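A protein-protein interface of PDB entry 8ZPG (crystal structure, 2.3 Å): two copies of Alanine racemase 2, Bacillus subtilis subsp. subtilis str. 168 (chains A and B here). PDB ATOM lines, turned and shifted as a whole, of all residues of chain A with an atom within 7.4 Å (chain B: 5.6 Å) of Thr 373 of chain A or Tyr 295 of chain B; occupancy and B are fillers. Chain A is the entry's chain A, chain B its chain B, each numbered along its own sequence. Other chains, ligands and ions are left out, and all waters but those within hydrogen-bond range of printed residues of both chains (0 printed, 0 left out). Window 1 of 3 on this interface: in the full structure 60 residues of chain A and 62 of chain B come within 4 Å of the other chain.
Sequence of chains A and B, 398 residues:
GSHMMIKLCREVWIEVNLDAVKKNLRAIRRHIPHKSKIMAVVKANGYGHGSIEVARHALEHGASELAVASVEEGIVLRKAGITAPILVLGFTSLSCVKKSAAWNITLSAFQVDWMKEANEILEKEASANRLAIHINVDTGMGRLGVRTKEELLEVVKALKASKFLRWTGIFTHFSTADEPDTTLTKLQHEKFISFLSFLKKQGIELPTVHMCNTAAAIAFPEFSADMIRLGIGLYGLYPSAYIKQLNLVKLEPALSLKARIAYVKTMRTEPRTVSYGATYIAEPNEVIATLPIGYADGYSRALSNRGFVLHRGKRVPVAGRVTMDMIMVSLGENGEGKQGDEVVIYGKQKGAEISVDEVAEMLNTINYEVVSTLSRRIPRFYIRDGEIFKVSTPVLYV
The backbone NH (N) of Arg 301 of chain B is in hydrogen-bond range of the side-chain carboxylate (OE2) of Glu 369 of chain A (3.1 Å).
The side-chain hydroxyl (OG1) of Thr 365 of chain A sits at hydrogen-bond distance from the side-chain carboxylate (OE1) of Glu 369 of chain A (2.7 Å).
The backbone carbonyl oxygen (O) of Tyr 368 of chain A lies within hydrogen-bond range of the side-chain hydroxyl (OG) of Ser 372 of chain A.
The backbone carbonyl oxygen (O) of Glu 369 of chain A lies within hydrogen-bond range of the side-chain hydroxyl (OG1) of Thr 373 of chain A, at 2.7 Å.
The backbone NH (N) of Tyr 295 of chain B lies within hydrogen-bond range of the backbone carbonyl oxygen (O) of Thr 323 of chain B (3.2 Å).
The backbone NH (N) of Tyr 295 of chain B sits at hydrogen-bond distance from the backbone carbonyl oxygen (O) of Met 324 of chain B (3.4 Å).
The backbone carbonyl oxygen (O) of Met 324 of chain B sits at hydrogen-bond distance from the backbone NH (N) of Ala 296 of chain B (3.3 Å).
SD of Met 324 of chain B touches CB of Ala 44 of chain A, 3.9 Å away.
Ile 366 of chain A touches Arg 301 of chain B (CD1 to NE, 3.2 Å).
Tyr 295 of chain B touches Tyr 368 of chain A.
Glu 369 of chain A touches Tyr 295 of chain B (OE2 to CB, 3.5 Å).
Glu 369 of chain A touches Ser 300 of chain B (OE2 to CA, 3.8 Å).
Ala 296 of chain B touches Ser 372 of chain A (CB to OG, 3.8 Å).
Ser 372 of chain A touches Met 324 of chain B.
Thr 373 of chain A touches Tyr 295 of chain B (CG2 to O, 3.5 Å).
Of the printed residues of chain B, Glu 369 of chain A touches Tyr 295, Ser 300 and Arg 301.
Thr 373 of chain A touches one residue of chain B.
Tyr 295 of chain B touches just these residues of chain A: Tyr 368, Glu 369 and Thr 373.
Of the printed residues of chain A, Met 324 of chain B touches Ala 44 (3.9 Å) and Ser 372 (3.9 Å).
The nearest residue of chain B that does not touch Thr 373 of chain A is Ala 296 of chain B (4.4 Å).
The nearest printed residue of chain A that does not touch Ala 296 of chain B is Ala 44 of chain A (4.04 Å).
Of the 23 printed residues of chain A, 6 touch a printed residue of chain B.
Hydrophobic or aromatic side chains of chain B that line the printed part of chain A: Tyr 295, Ala 296 and Met 324.
Among the printed residues, 9 pairs touch across the chains.
Among the printed residues, no Asp or Glu carboxylate lies within 4 Å of a Lys or Arg side-chain nitrogen of the other chain.
Positions printed for both chains: 295, 296, 297, 298 and 299.
Of the 9 pairs that touch across the chains among the printed residues, none has its exchanged pair printed and touching as well.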
ATOM      1  N   ALA A  44     -16.028  20.002  19.329  1.00  0.00           N
ATOM      2  CA  ALA A  44     -16.443  20.481  20.653  1.00  0.00           C
ATOM      3  C   ALA A  44     -17.556  19.624  21.273  1.00  0.00           C
ATOM      4  O   ALA A  44     -18.526  20.145  21.838  1.00  0.00           O
ATOM      5  CB  ALA A  44     -16.882  21.939  20.581  1.00  0.00           C
ATOM      6  N   TYR A  47     -21.003  20.135  19.487  1.00  0.00           N
ATOM      7  CA  TYR A  47     -21.581  21.409  19.897  1.00  0.00           C
ATOM      8  C   TYR A  47     -22.340  21.271  21.222  1.00  0.00           C
ATOM      9  O   TYR A  47     -23.388  21.892  21.433  1.00  0.00           O
ATOM     10  CB  TYR A  47     -22.486  21.984  18.803  1.00  0.00           C
ATOM     11  CG  TYR A  47     -21.780  22.499  17.543  1.00  0.00           C
ATOM     12  CD1 TYR A  47     -20.558  21.967  17.100  1.00  0.00           C
ATOM     13  CD2 TYR A  47     -22.363  23.502  16.777  1.00  0.00           C
ATOM     14  CE1 TYR A  47     -19.939  22.452  15.933  1.00  0.00           C
ATOM     15  CE2 TYR A  47     -21.763  23.986  15.614  1.00  0.00           C
ATOM     16  CZ  TYR A  47     -20.558  23.474  15.196  1.00  0.00           C
ATOM     17  OH  TYR A  47     -20.007  24.000  14.032  1.00  0.00           O
ATOM     18  N   GLY A  48     -21.804  20.453  22.136  1.00  0.00           N
ATOM     19  CA  GLY A  48     -22.419  20.272  23.438  1.00  0.00           C
ATOM     20  C   GLY A  48     -23.506  19.212  23.512  1.00  0.00           C
ATOM     21  O   GLY A  48     -24.008  18.950  24.625  1.00  0.00           O
ATOM     22  N   TYR A 295     -23.701  28.072  38.147  1.00  0.00           N
ATOM     23  CA  TYR A 295     -22.845  28.583  37.069  1.00  0.00           C
ATOM     24  C   TYR A 295     -21.717  27.617  36.688  1.00  0.00           C
ATOM     25  O   TYR A 295     -21.237  27.673  35.549  1.00  0.00           O
ATOM     26  CB  TYR A 295     -22.290  29.988  37.408  1.00  0.00           C
ATOM     27  CG  TYR A 295     -21.525  30.160  38.731  1.00  0.00           C
ATOM     28  CD1 TYR A 295     -20.218  29.677  38.873  1.00  0.00           C
ATOM     29  CD2 TYR A 295     -22.094  30.843  39.816  1.00  0.00           C
ATOM     30  CE1 TYR A 295     -19.516  29.828  40.055  1.00  0.00           C
ATOM     31  CE2 TYR A 295     -21.405  30.987  41.023  1.00  0.00           C
ATOM     32  CZ  TYR A 295     -20.107  30.470  41.135  1.00  0.00           C
ATOM     33  OH  TYR A 295     -19.379  30.599  42.306  1.00  0.00           O
ATOM     34  N   ALA A 296     -21.298  26.705  37.578  1.00  0.00           N
ATOM     35  CA  ALA A 296     -20.269  25.749  37.153  1.00  0.00           C
ATOM     36  C   ALA A 296     -20.801  24.689  36.182  1.00  0.00           C
ATOM     37  O   ALA A 296     -19.993  23.968  35.582  1.00  0.00           O
ATOM     38  CB  ALA A 296     -19.621  25.060  38.360  1.00  0.00           C
ATOM     39  N   ASP A 297     -22.127  24.595  36.002  1.00  0.00           N
ATOM     40  CA  ASP A 297     -22.761  23.755  34.989  1.00  0.00           C
ATOM     41  C   ASP A 297     -22.863  24.434  33.622  1.00  0.00           C
ATOM     42  O   ASP A 297     -23.177  23.745  32.628  1.00  0.00           O
ATOM     43  CB  ASP A 297     -24.179  23.370  35.425  1.00  0.00           C
ATOM     44  CG  ASP A 297     -24.204  22.547  36.695  1.00  0.00           C
ATOM     45  OD1 ASP A 297     -23.714  21.394  36.664  1.00  0.00           O
ATOM     46  OD2 ASP A 297     -24.738  23.035  37.719  1.00  0.00           O
ATOM     47  N   GLY A 298     -22.649  25.763  33.565  1.00  0.00           N
ATOM     48  CA  GLY A 298     -22.885  26.569  32.379  1.00  0.00           C
ATOM     49  C   GLY A 298     -24.086  27.511  32.418  1.00  0.00           C
ATOM     50  O   GLY A 298     -24.338  28.176  31.410  1.00  0.00           O
ATOM     51  N   TYR A 299     -24.829  27.602  33.528  1.00  0.00           N
ATOM     52  CA  TYR A 299     -25.900  28.587  33.697  1.00  0.00           C
ATOM     53  C   TYR A 299     -25.294  29.895  34.210  1.00  0.00           C
ATOM     54  O   TYR A 299     -24.797  29.961  35.339  1.00  0.00           O
ATOM     55  CB  TYR A 299     -26.974  28.068  34.653  1.00  0.00           C
ATOM     56  CG  TYR A 299     -28.311  28.813  34.566  1.00  0.00           C
ATOM     57  CD1 TYR A 299     -29.190  28.606  33.495  1.00  0.00           C
ATOM     58  CD2 TYR A 299     -28.687  29.722  35.550  1.00  0.00           C
ATOM     59  CE1 TYR A 299     -30.403  29.279  33.419  1.00  0.00           C
ATOM     60  CE2 TYR A 299     -29.893  30.410  35.474  1.00  0.00           C
ATOM     61  CZ  TYR A 299     -30.747  30.187  34.413  1.00  0.00           C
ATOM     62  OH  TYR A 299     -31.940  30.889  34.357  1.00  0.00           O
ATOM     63  N   TYR A 346     -34.188  25.076  29.523  1.00  0.00           N
ATOM     64  CA  TYR A 346     -34.273  25.394  28.093  1.00  0.00           C
ATOM     65  C   TYR A 346     -35.249  24.431  27.417  1.00  0.00           C
ATOM     66  O   TYR A 346     -35.107  23.208  27.562  1.00  0.00           O
ATOM     67  CB  TYR A 346     -32.915  25.284  27.356  1.00  0.00           C
ATOM     68  CG  TYR A 346     -31.715  26.080  27.881  1.00  0.00           C
ATOM     69  CD1 TYR A 346     -31.870  27.266  28.594  1.00  0.00           C
ATOM     70  CD2 TYR A 346     -30.413  25.650  27.613  1.00  0.00           C
ATOM     71  CE1 TYR A 346     -30.758  27.973  29.051  1.00  0.00           C
ATOM     72  CE2 TYR A 346     -29.314  26.342  28.069  1.00  0.00           C
ATOM     73  CZ  TYR A 346     -29.494  27.494  28.788  1.00  0.00           C
ATOM     74  OH  TYR A 346     -28.389  28.172  29.239  1.00  0.00           O
ATOM     75  N   THR A 365     -24.783  37.432  23.240  1.00  0.00           N
ATOM     76  CA  THR A 365     -23.875  36.455  22.650  1.00  0.00           C
ATOM     77  C   THR A 365     -24.641  35.750  21.527  1.00  0.00           C
ATOM     78  O   THR A 365     -25.610  36.294  20.984  1.00  0.00           O
ATOM     79  CB  THR A 365     -23.298  35.543  23.759  1.00  0.00           C
ATOM     80  OG1 THR A 365     -22.274  34.722  23.207  1.00  0.00           O
ATOM     81  CG2 THR A 365     -24.367  34.663  24.408  1.00  0.00           C
ATOM     82  N   ILE A 366     -24.215  34.534  21.145  1.00  0.00           N
ATOM     83  CA  ILE A 366     -24.825  33.809  20.032  1.00  0.00           C
ATOM     84  C   ILE A 366     -25.143  32.391  20.474  1.00  0.00           C
ATOM     85  O   ILE A 366     -24.498  31.854  21.384  1.00  0.00           O
ATOM     86  CB  ILE A 366     -23.902  33.803  18.791  1.00  0.00           C
ATOM     87  CG1 ILE A 366     -22.500  33.277  19.143  1.00  0.00           C
ATOM     88  CG2 ILE A 366     -23.782  35.205  18.213  1.00  0.00           C
ATOM     89  CD1 ILE A 366     -21.536  33.280  17.940  1.00  0.00           C
ATOM     90  N   ASN A 367     -26.137  31.765  19.821  1.00  0.00           N
ATOM     91  CA  ASN A 367     -26.582  30.453  20.296  1.00  0.00           C
ATOM     92  C   ASN A 367     -25.435  29.437  20.316  1.00  0.00           C
ATOM     93  O   ASN A 367     -25.369  28.592  21.224  1.00  0.00           O
ATOM     94  CB  ASN A 367     -27.783  29.947  19.471  1.00  0.00           C
ATOM     95  CG  ASN A 367     -27.515  29.924  17.968  1.00  0.00           C
ATOM     96  OD1 ASN A 367     -26.371  29.993  17.529  1.00  0.00           O
ATOM     97  ND2 ASN A 367     -28.584  29.838  17.172  1.00  0.00           N
ATOM     98  N   TYR A 368     -24.505  29.529  19.356  1.00  0.00           N
ATOM     99  CA  TYR A 368     -23.296  28.700  19.350  1.00  0.00           C
ATOM    100  C   TYR A 368     -22.645  28.557  20.740  1.00  0.00           C
ATOM    101  O   TYR A 368     -22.276  27.458  21.149  1.00  0.00           O
ATOM    102  CB  TYR A 368     -22.258  29.281  18.387  1.00  0.00           C
ATOM    103  CG  TYR A 368     -22.495  29.216  16.869  1.00  0.00           C
ATOM    104  CD1 TYR A 368     -23.356  30.117  16.234  1.00  0.00           C
ATOM    105  CD2 TYR A 368     -21.778  28.303  16.063  1.00  0.00           C
ATOM    106  CE1 TYR A 368     -23.527  30.095  14.828  1.00  0.00           C
ATOM    107  CE2 TYR A 368     -21.946  28.257  14.687  1.00  0.00           C
ATOM    108  CZ  TYR A 368     -22.824  29.161  14.065  1.00  0.00           C
ATOM    109  OH  TYR A 368     -22.974  29.140  12.684  1.00  0.00           O
ATOM    110  N   GLU A 369     -22.459  29.655  21.465  1.00  0.00           N
ATOM    111  CA  GLU A 369     -21.738  29.599  22.737  1.00  0.00           C
ATOM    112  C   GLU A 369     -22.593  29.047  23.876  1.00  0.00           C
ATOM    113  O   GLU A 369     -22.045  28.535  24.868  1.00  0.00           O
ATOM    114  CB  GLU A 369     -21.197  31.002  23.122  1.00  0.00           C
ATOM    115  CG  GLU A 369     -20.413  31.048  24.493  1.00  0.00           C
ATOM    116  CD  GLU A 369     -19.746  32.421  24.814  1.00  0.00           C
ATOM    117  OE1 GLU A 369     -20.405  33.474  24.679  1.00  0.00           O
ATOM    118  OE2 GLU A 369     -18.557  32.446  25.218  1.00  0.00           O
ATOM    119  N   VAL A 370     -23.914  29.160  23.761  1.00  0.00           N
ATOM    120  CA  VAL A 370     -24.808  28.780  24.850  1.00  0.00           C
ATOM    121  C   VAL A 370     -24.886  27.270  24.982  1.00  0.00           C
ATOM    122  O   VAL A 370     -24.976  26.746  26.097  1.00  0.00           O
ATOM    123  CB  VAL A 370     -26.206  29.393  24.644  1.00  0.00           C
ATOM    124  CG1 VAL A 370     -27.217  28.760  25.601  1.00  0.00           C
ATOM    125  CG2 VAL A 370     -26.144  30.920  24.819  1.00  0.00           C
ATOM    126  N   VAL A 371     -24.854  26.548  23.860  1.00  0.00           N
ATOM    127  CA  VAL A 371     -24.920  25.093  23.924  1.00  0.00           C
ATOM    128  C   VAL A 371     -23.538  24.479  24.109  1.00  0.00           C
ATOM    129  O   VAL A 371     -23.396  23.491  24.825  1.00  0.00           O
ATOM    130  CB  VAL A 371     -25.625  24.508  22.680  1.00  0.00           C
ATOM    131  CG1 VAL A 371     -27.140  24.719  22.767  1.00  0.00           C
ATOM    132  CG2 VAL A 371     -25.041  25.065  21.375  1.00  0.00           C
ATOM    133  N   SER A 372     -22.483  25.004  23.480  1.00  0.00           N
ATOM    134  CA  SER A 372     -21.246  24.239  23.537  1.00  0.00           C
ATOM    135  C   SER A 372     -20.449  24.506  24.805  1.00  0.00           C
ATOM    136  O   SER A 372     -19.357  23.950  24.956  1.00  0.00           O
ATOM    137  CB  SER A 372     -20.385  24.495  22.297  1.00  0.00           C
ATOM    138  OG  SER A 372     -19.934  25.834  22.241  1.00  0.00           O
ATOM    139  N   THR A 373     -20.970  25.320  25.727  1.00  0.00           N
ATOM    140  CA  THR A 373     -20.368  25.492  27.045  1.00  0.00           C
ATOM    141  C   THR A 373     -21.149  24.778  28.159  1.00  0.00           C
ATOM    142  O   THR A 373     -20.956  25.088  29.338  1.00  0.00           O
ATOM    143  CB  THR A 373     -20.213  26.982  27.355  1.00  0.00           C
ATOM    144  OG1 THR A 373     -21.500  27.632  27.317  1.00  0.00           O
ATOM    145  CG2 THR A 373     -19.278  27.625  26.317  1.00  0.00           C
ATOM    146  N   LEU A 374     -22.002  23.810  27.812  1.00  0.00           N
ATOM    147  CA  LEU A 374     -22.696  22.974  28.791  1.00  0.00           C
ATOM    148  C   LEU A 374     -21.759  21.871  29.310  1.00  0.00           C
ATOM    149  O   LEU A 374     -21.262  21.045  28.531  1.00  0.00           O
ATOM    150  CB  LEU A 374     -23.958  22.377  28.163  1.00  0.00           C
ATOM    151  CG  LEU A 374     -25.148  23.339  28.021  1.00  0.00           C
ATOM    152  CD1 LEU A 374     -26.311  22.654  27.342  1.00  0.00           C
ATOM    153  CD2 LEU A 374     -25.598  23.926  29.347  1.00  0.00           C
ATOM    154  N   SER A 375     -21.529  21.866  30.627  1.00  0.00           N
ATOM    155  CA  SER A 375     -20.541  20.999  31.260  1.00  0.00           C
ATOM    156  C   SER A 375     -20.789  19.518  30.960  1.00  0.00           C
ATOM    157  O   SER A 375     -21.922  19.061  30.850  1.00  0.00           O
ATOM    158  CB  SER A 375     -20.562  21.224  32.777  1.00  0.00           C
ATOM    159  OG  SER A 375     -19.632  20.393  33.478  1.00  0.00           O
ATOM    160  N   ARG A 376     -19.703  18.749  30.877  1.00  0.00           N
ATOM    161  CA  ARG A 376     -19.837  17.306  30.711  1.00  0.00           C
ATOM    162  C   ARG A 376     -20.318  16.600  31.976  1.00  0.00           C
ATOM    163  O   ARG A 376     -20.630  15.405  31.905  1.00  0.00           O
ATOM    164  CB  ARG A 376     -18.508  16.688  30.269  1.00  0.00           C
ATOM    165  CG  ARG A 376     -18.195  16.785  28.774  1.00  0.00           C
ATOM    166  CD  ARG A 376     -16.721  16.399  28.558  1.00  0.00           C
ATOM    167  NE  ARG A 376     -16.191  16.763  27.246  1.00  0.00           N
ATOM    168  CZ  ARG A 376     -16.223  17.988  26.730  1.00  0.00           C
ATOM    169  NH1 ARG A 376     -16.856  18.987  27.345  1.00  0.00           N
ATOM    170  NH2 ARG A 376     -15.609  18.219  25.567  1.00  0.00           N
ATOM    171  N   ILE A 378     -23.111  17.096  33.356  1.00  0.00           N
ATOM    172  CA  ILE A 378     -24.554  16.907  33.182  1.00  0.00           C
ATOM    173  C   ILE A 378     -24.761  15.684  32.300  1.00  0.00           C
ATOM    174  O   ILE A 378     -24.252  15.658  31.163  1.00  0.00           O
ATOM    175  CB  ILE A 378     -25.237  18.123  32.543  1.00  0.00           C
ATOM    176  CG1 ILE A 378     -25.051  19.421  33.331  1.00  0.00           C
ATOM    177  CG2 ILE A 378     -26.753  17.833  32.331  1.00  0.00           C
ATOM    178  CD1 ILE A 378     -25.600  20.673  32.525  1.00  0.00           C
ATOM    179  N   ARG A 380     -26.462  13.121  29.597  1.00  0.00           N
ATOM    180  CA  ARG A 380     -27.202  13.291  28.343  1.00  0.00           C
ATOM    181  C   ARG A 380     -28.009  12.031  27.999  1.00  0.00           C
ATOM    182  O   ARG A 380     -27.458  10.926  27.984  1.00  0.00           O
ATOM    183  CB  ARG A 380     -26.240  13.597  27.186  1.00  0.00           C
ATOM    184  CG  ARG A 380     -25.837  15.049  27.030  1.00  0.00           C
ATOM    185  CD  ARG A 380     -24.334  15.235  27.118  1.00  0.00           C
ATOM    186  NE  ARG A 380     -23.925  16.601  26.844  1.00  0.00           N
ATOM    187  CZ  ARG A 380     -23.499  17.462  27.759  1.00  0.00           C
ATOM    188  NH1 ARG A 380     -23.479  17.148  29.048  1.00  0.00           N
ATOM    189  NH2 ARG A 380     -23.078  18.665  27.372  1.00  0.00           N
ATOM    190  N   ILE B 293      -7.053  28.224  21.126  1.00  0.00           N
ATOM    191  CA  ILE B 293      -8.021  28.252  22.220  1.00  0.00           C
ATOM    192  C   ILE B 293      -9.192  29.134  21.779  1.00  0.00           C
ATOM    193  O   ILE B 293      -9.034  30.003  20.914  1.00  0.00           O
ATOM    194  CB  ILE B 293      -7.396  28.737  23.551  1.00  0.00           C
ATOM    195  CG1 ILE B 293      -8.385  28.555  24.700  1.00  0.00           C
ATOM    196  CG2 ILE B 293      -7.003  30.205  23.476  1.00  0.00           C
ATOM    197  CD1 ILE B 293      -7.877  29.094  25.996  1.00  0.00           C
ATOM    198  N   GLY B 294     -10.383  28.870  22.339  1.00  0.00           N
ATOM    199  CA  GLY B 294     -11.636  29.468  21.885  1.00  0.00           C
ATOM    200  C   GLY B 294     -12.722  29.393  22.945  1.00  0.00           C
ATOM    201  O   GLY B 294     -12.495  28.910  24.058  1.00  0.00           O
ATOM    202  N   TYR B 295     -13.935  29.860  22.589  1.00  0.00           N
ATOM    203  CA  TYR B 295     -14.966  29.994  23.620  1.00  0.00           C
ATOM    204  C   TYR B 295     -15.560  28.652  24.062  1.00  0.00           C
ATOM    205  O   TYR B 295     -16.145  28.571  25.153  1.00  0.00           O
ATOM    206  CB  TYR B 295     -16.081  30.960  23.182  1.00  0.00           C
ATOM    207  CG  TYR B 295     -16.865  30.626  21.911  1.00  0.00           C
ATOM    208  CD1 TYR B 295     -17.867  29.641  21.911  1.00  0.00           C
ATOM    209  CD2 TYR B 295     -16.642  31.347  20.724  1.00  0.00           C
ATOM    210  CE1 TYR B 295     -18.595  29.349  20.759  1.00  0.00           C
ATOM    211  CE2 TYR B 295     -17.364  31.065  19.545  1.00  0.00           C
ATOM    212  CZ  TYR B 295     -18.339  30.062  19.576  1.00  0.00           C
ATOM    213  OH  TYR B 295     -19.055  29.773  18.435  1.00  0.00           O
ATOM    214  N   ALA B 296     -15.419  27.592  23.276  1.00  0.00           N
ATOM    215  CA  ALA B 296     -15.877  26.315  23.805  1.00  0.00           C
ATOM    216  C   ALA B 296     -14.885  25.729  24.799  1.00  0.00           C
ATOM    217  O   ALA B 296     -15.216  24.758  25.482  1.00  0.00           O
ATOM    218  CB  ALA B 296     -16.160  25.320  22.674  1.00  0.00           C
ATOM    219  N   ASP B 297     -13.679  26.303  24.906  1.00  0.00           N
ATOM    220  CA  ASP B 297     -12.781  25.936  25.992  1.00  0.00           C
ATOM    221  C   ASP B 297     -13.125  26.676  27.279  1.00  0.00           C
ATOM    222  O   ASP B 297     -12.727  26.225  28.362  1.00  0.00           O
ATOM    223  CB  ASP B 297     -11.320  26.202  25.602  1.00  0.00           C
ATOM    224  CG  ASP B 297     -10.903  25.466  24.353  1.00  0.00           C
ATOM    225  OD1 ASP B 297     -10.714  24.224  24.395  1.00  0.00           O
ATOM    226  OD2 ASP B 297     -10.756  26.128  23.307  1.00  0.00           O
ATOM    227  N   GLY B 298     -13.864  27.795  27.178  1.00  0.00           N
ATOM    228  CA  GLY B 298     -14.216  28.614  28.324  1.00  0.00           C
ATOM    229  C   GLY B 298     -13.658  30.026  28.296  1.00  0.00           C
ATOM    230  O   GLY B 298     -13.766  30.751  29.297  1.00  0.00           O
ATOM    231  N   TYR B 299     -13.070  30.432  27.159  1.00  0.00           N
ATOM    232  CA  TYR B 299     -12.545  31.784  26.969  1.00  0.00           C
ATOM    233  C   TYR B 299     -13.664  32.631  26.346  1.00  0.00           C
ATOM    234  O   TYR B 299     -13.942  32.554  25.145  1.00  0.00           O
ATOM    235  CB  TYR B 299     -11.269  31.726  26.130  1.00  0.00           C
ATOM    236  CG  TYR B 299     -10.416  32.983  26.128  1.00  0.00           C
ATOM    237  CD1 TYR B 299      -9.703  33.388  27.255  1.00  0.00           C
ATOM    238  CD2 TYR B 299     -10.311  33.760  24.976  1.00  0.00           C
ATOM    239  CE1 TYR B 299      -8.912  34.547  27.227  1.00  0.00           C
ATOM    240  CE2 TYR B 299      -9.543  34.901  24.942  1.00  0.00           C
ATOM    241  CZ  TYR B 299      -8.843  35.295  26.059  1.00  0.00           C
ATOM    242  OH  TYR B 299      -8.089  36.453  25.971  1.00  0.00           O
ATOM    243  N   SER B 300     -14.312  33.448  27.177  1.00  0.00           N
ATOM    244  CA  SER B 300     -15.548  34.136  26.805  1.00  0.00           C
ATOM    245  C   SER B 300     -15.455  34.850  25.459  1.00  0.00           C
ATOM    246  O   SER B 300     -14.526  35.623  25.206  1.00  0.00           O
ATOM    247  CB  SER B 300     -15.911  35.148  27.893  1.00  0.00           C
ATOM    248  OG  SER B 300     -17.144  35.796  27.597  1.00  0.00           O
ATOM    249  N   ARG B 301     -16.466  34.628  24.617  1.00  0.00           N
ATOM    250  CA  ARG B 301     -16.627  35.427  23.405  1.00  0.00           C
ATOM    251  C   ARG B 301     -16.633  36.933  23.697  1.00  0.00           C
ATOM    252  O   ARG B 301     -16.302  37.741  22.811  1.00  0.00           O
ATOM    253  CB  ARG B 301     -17.916  35.027  22.701  1.00  0.00           C
ATOM    254  CG  ARG B 301     -17.968  35.384  21.229  1.00  0.00           C
ATOM    255  CD  ARG B 301     -19.182  34.765  20.577  1.00  0.00           C
ATOM    256  NE  ARG B 301     -19.520  35.398  19.303  1.00  0.00           N
ATOM    257  CZ  ARG B 301     -20.235  36.509  19.174  1.00  0.00           C
ATOM    258  NH1 ARG B 301     -20.728  37.147  20.230  1.00  0.00           N
ATOM    259  NH2 ARG B 301     -20.451  37.001  17.956  1.00  0.00           N
ATOM    260  N   VAL B 322     -13.512  36.342  18.744  1.00  0.00           N
ATOM    261  CA  VAL B 322     -13.209  34.991  19.222  1.00  0.00           C
ATOM    262  C   VAL B 322     -14.093  33.979  18.479  1.00  0.00           C
ATOM    263  O   VAL B 322     -15.284  34.233  18.242  1.00  0.00           O
ATOM    264  CB  VAL B 322     -13.443  34.940  20.749  1.00  0.00           C
ATOM    265  CG1 VAL B 322     -13.191  33.537  21.350  1.00  0.00           C
ATOM    266  CG2 VAL B 322     -12.597  35.965  21.445  1.00  0.00           C
ATOM    267  N   THR B 323     -13.522  32.824  18.109  1.00  0.00           N
ATOM    268  CA  THR B 323     -14.285  31.722  17.495  1.00  0.00           C
ATOM    269  C   THR B 323     -14.225  30.471  18.379  1.00  0.00           C
ATOM    270  O   THR B 323     -13.625  30.470  19.459  1.00  0.00           O
ATOM    271  CB  THR B 323     -13.802  31.399  16.075  1.00  0.00           C
ATOM    272  OG1 THR B 323     -12.669  30.520  16.123  1.00  0.00           O
ATOM    273  CG2 THR B 323     -13.445  32.679  15.294  1.00  0.00           C
ATOM    274  N   MET B 324     -14.862  29.392  17.907  1.00  0.00           N
ATOM    275  CA  MET B 324     -15.141  28.255  18.786  1.00  0.00           C
ATOM    276  C   MET B 324     -13.853  27.616  19.315  1.00  0.00           C
ATOM    277  O   MET B 324     -13.788  27.218  20.486  1.00  0.00           O
ATOM    278  CB  MET B 324     -16.004  27.218  18.053  1.00  0.00           C
ATOM    279  CG  MET B 324     -16.336  25.959  18.843  1.00  0.00           C
ATOM    280  SD  MET B 324     -17.806  24.997  18.282  1.00  0.00           S
ATOM    281  CE  MET B 324     -19.155  26.158  18.419  1.00  0.00           C
ATOM    282  N   ASP B 325     -12.807  27.536  18.478  1.00  0.00           N
ATOM    283  CA  ASP B 325     -11.602  26.786  18.808  1.00  0.00           C
ATOM    284  C   ASP B 325     -10.310  27.567  18.642  1.00  0.00           C
ATOM    285  O   ASP B 325      -9.239  26.992  18.867  1.00  0.00           O
ATOM    286  CB  ASP B 325     -11.486  25.511  17.951  1.00  0.00           C
ATOM    287  CG  ASP B 325     -12.730  24.644  17.995  1.00  0.00           C
ATOM    288  OD1 ASP B 325     -13.201  24.310  19.107  1.00  0.00           O
ATOM    289  OD2 ASP B 325     -13.231  24.262  16.916  1.00  0.00           O
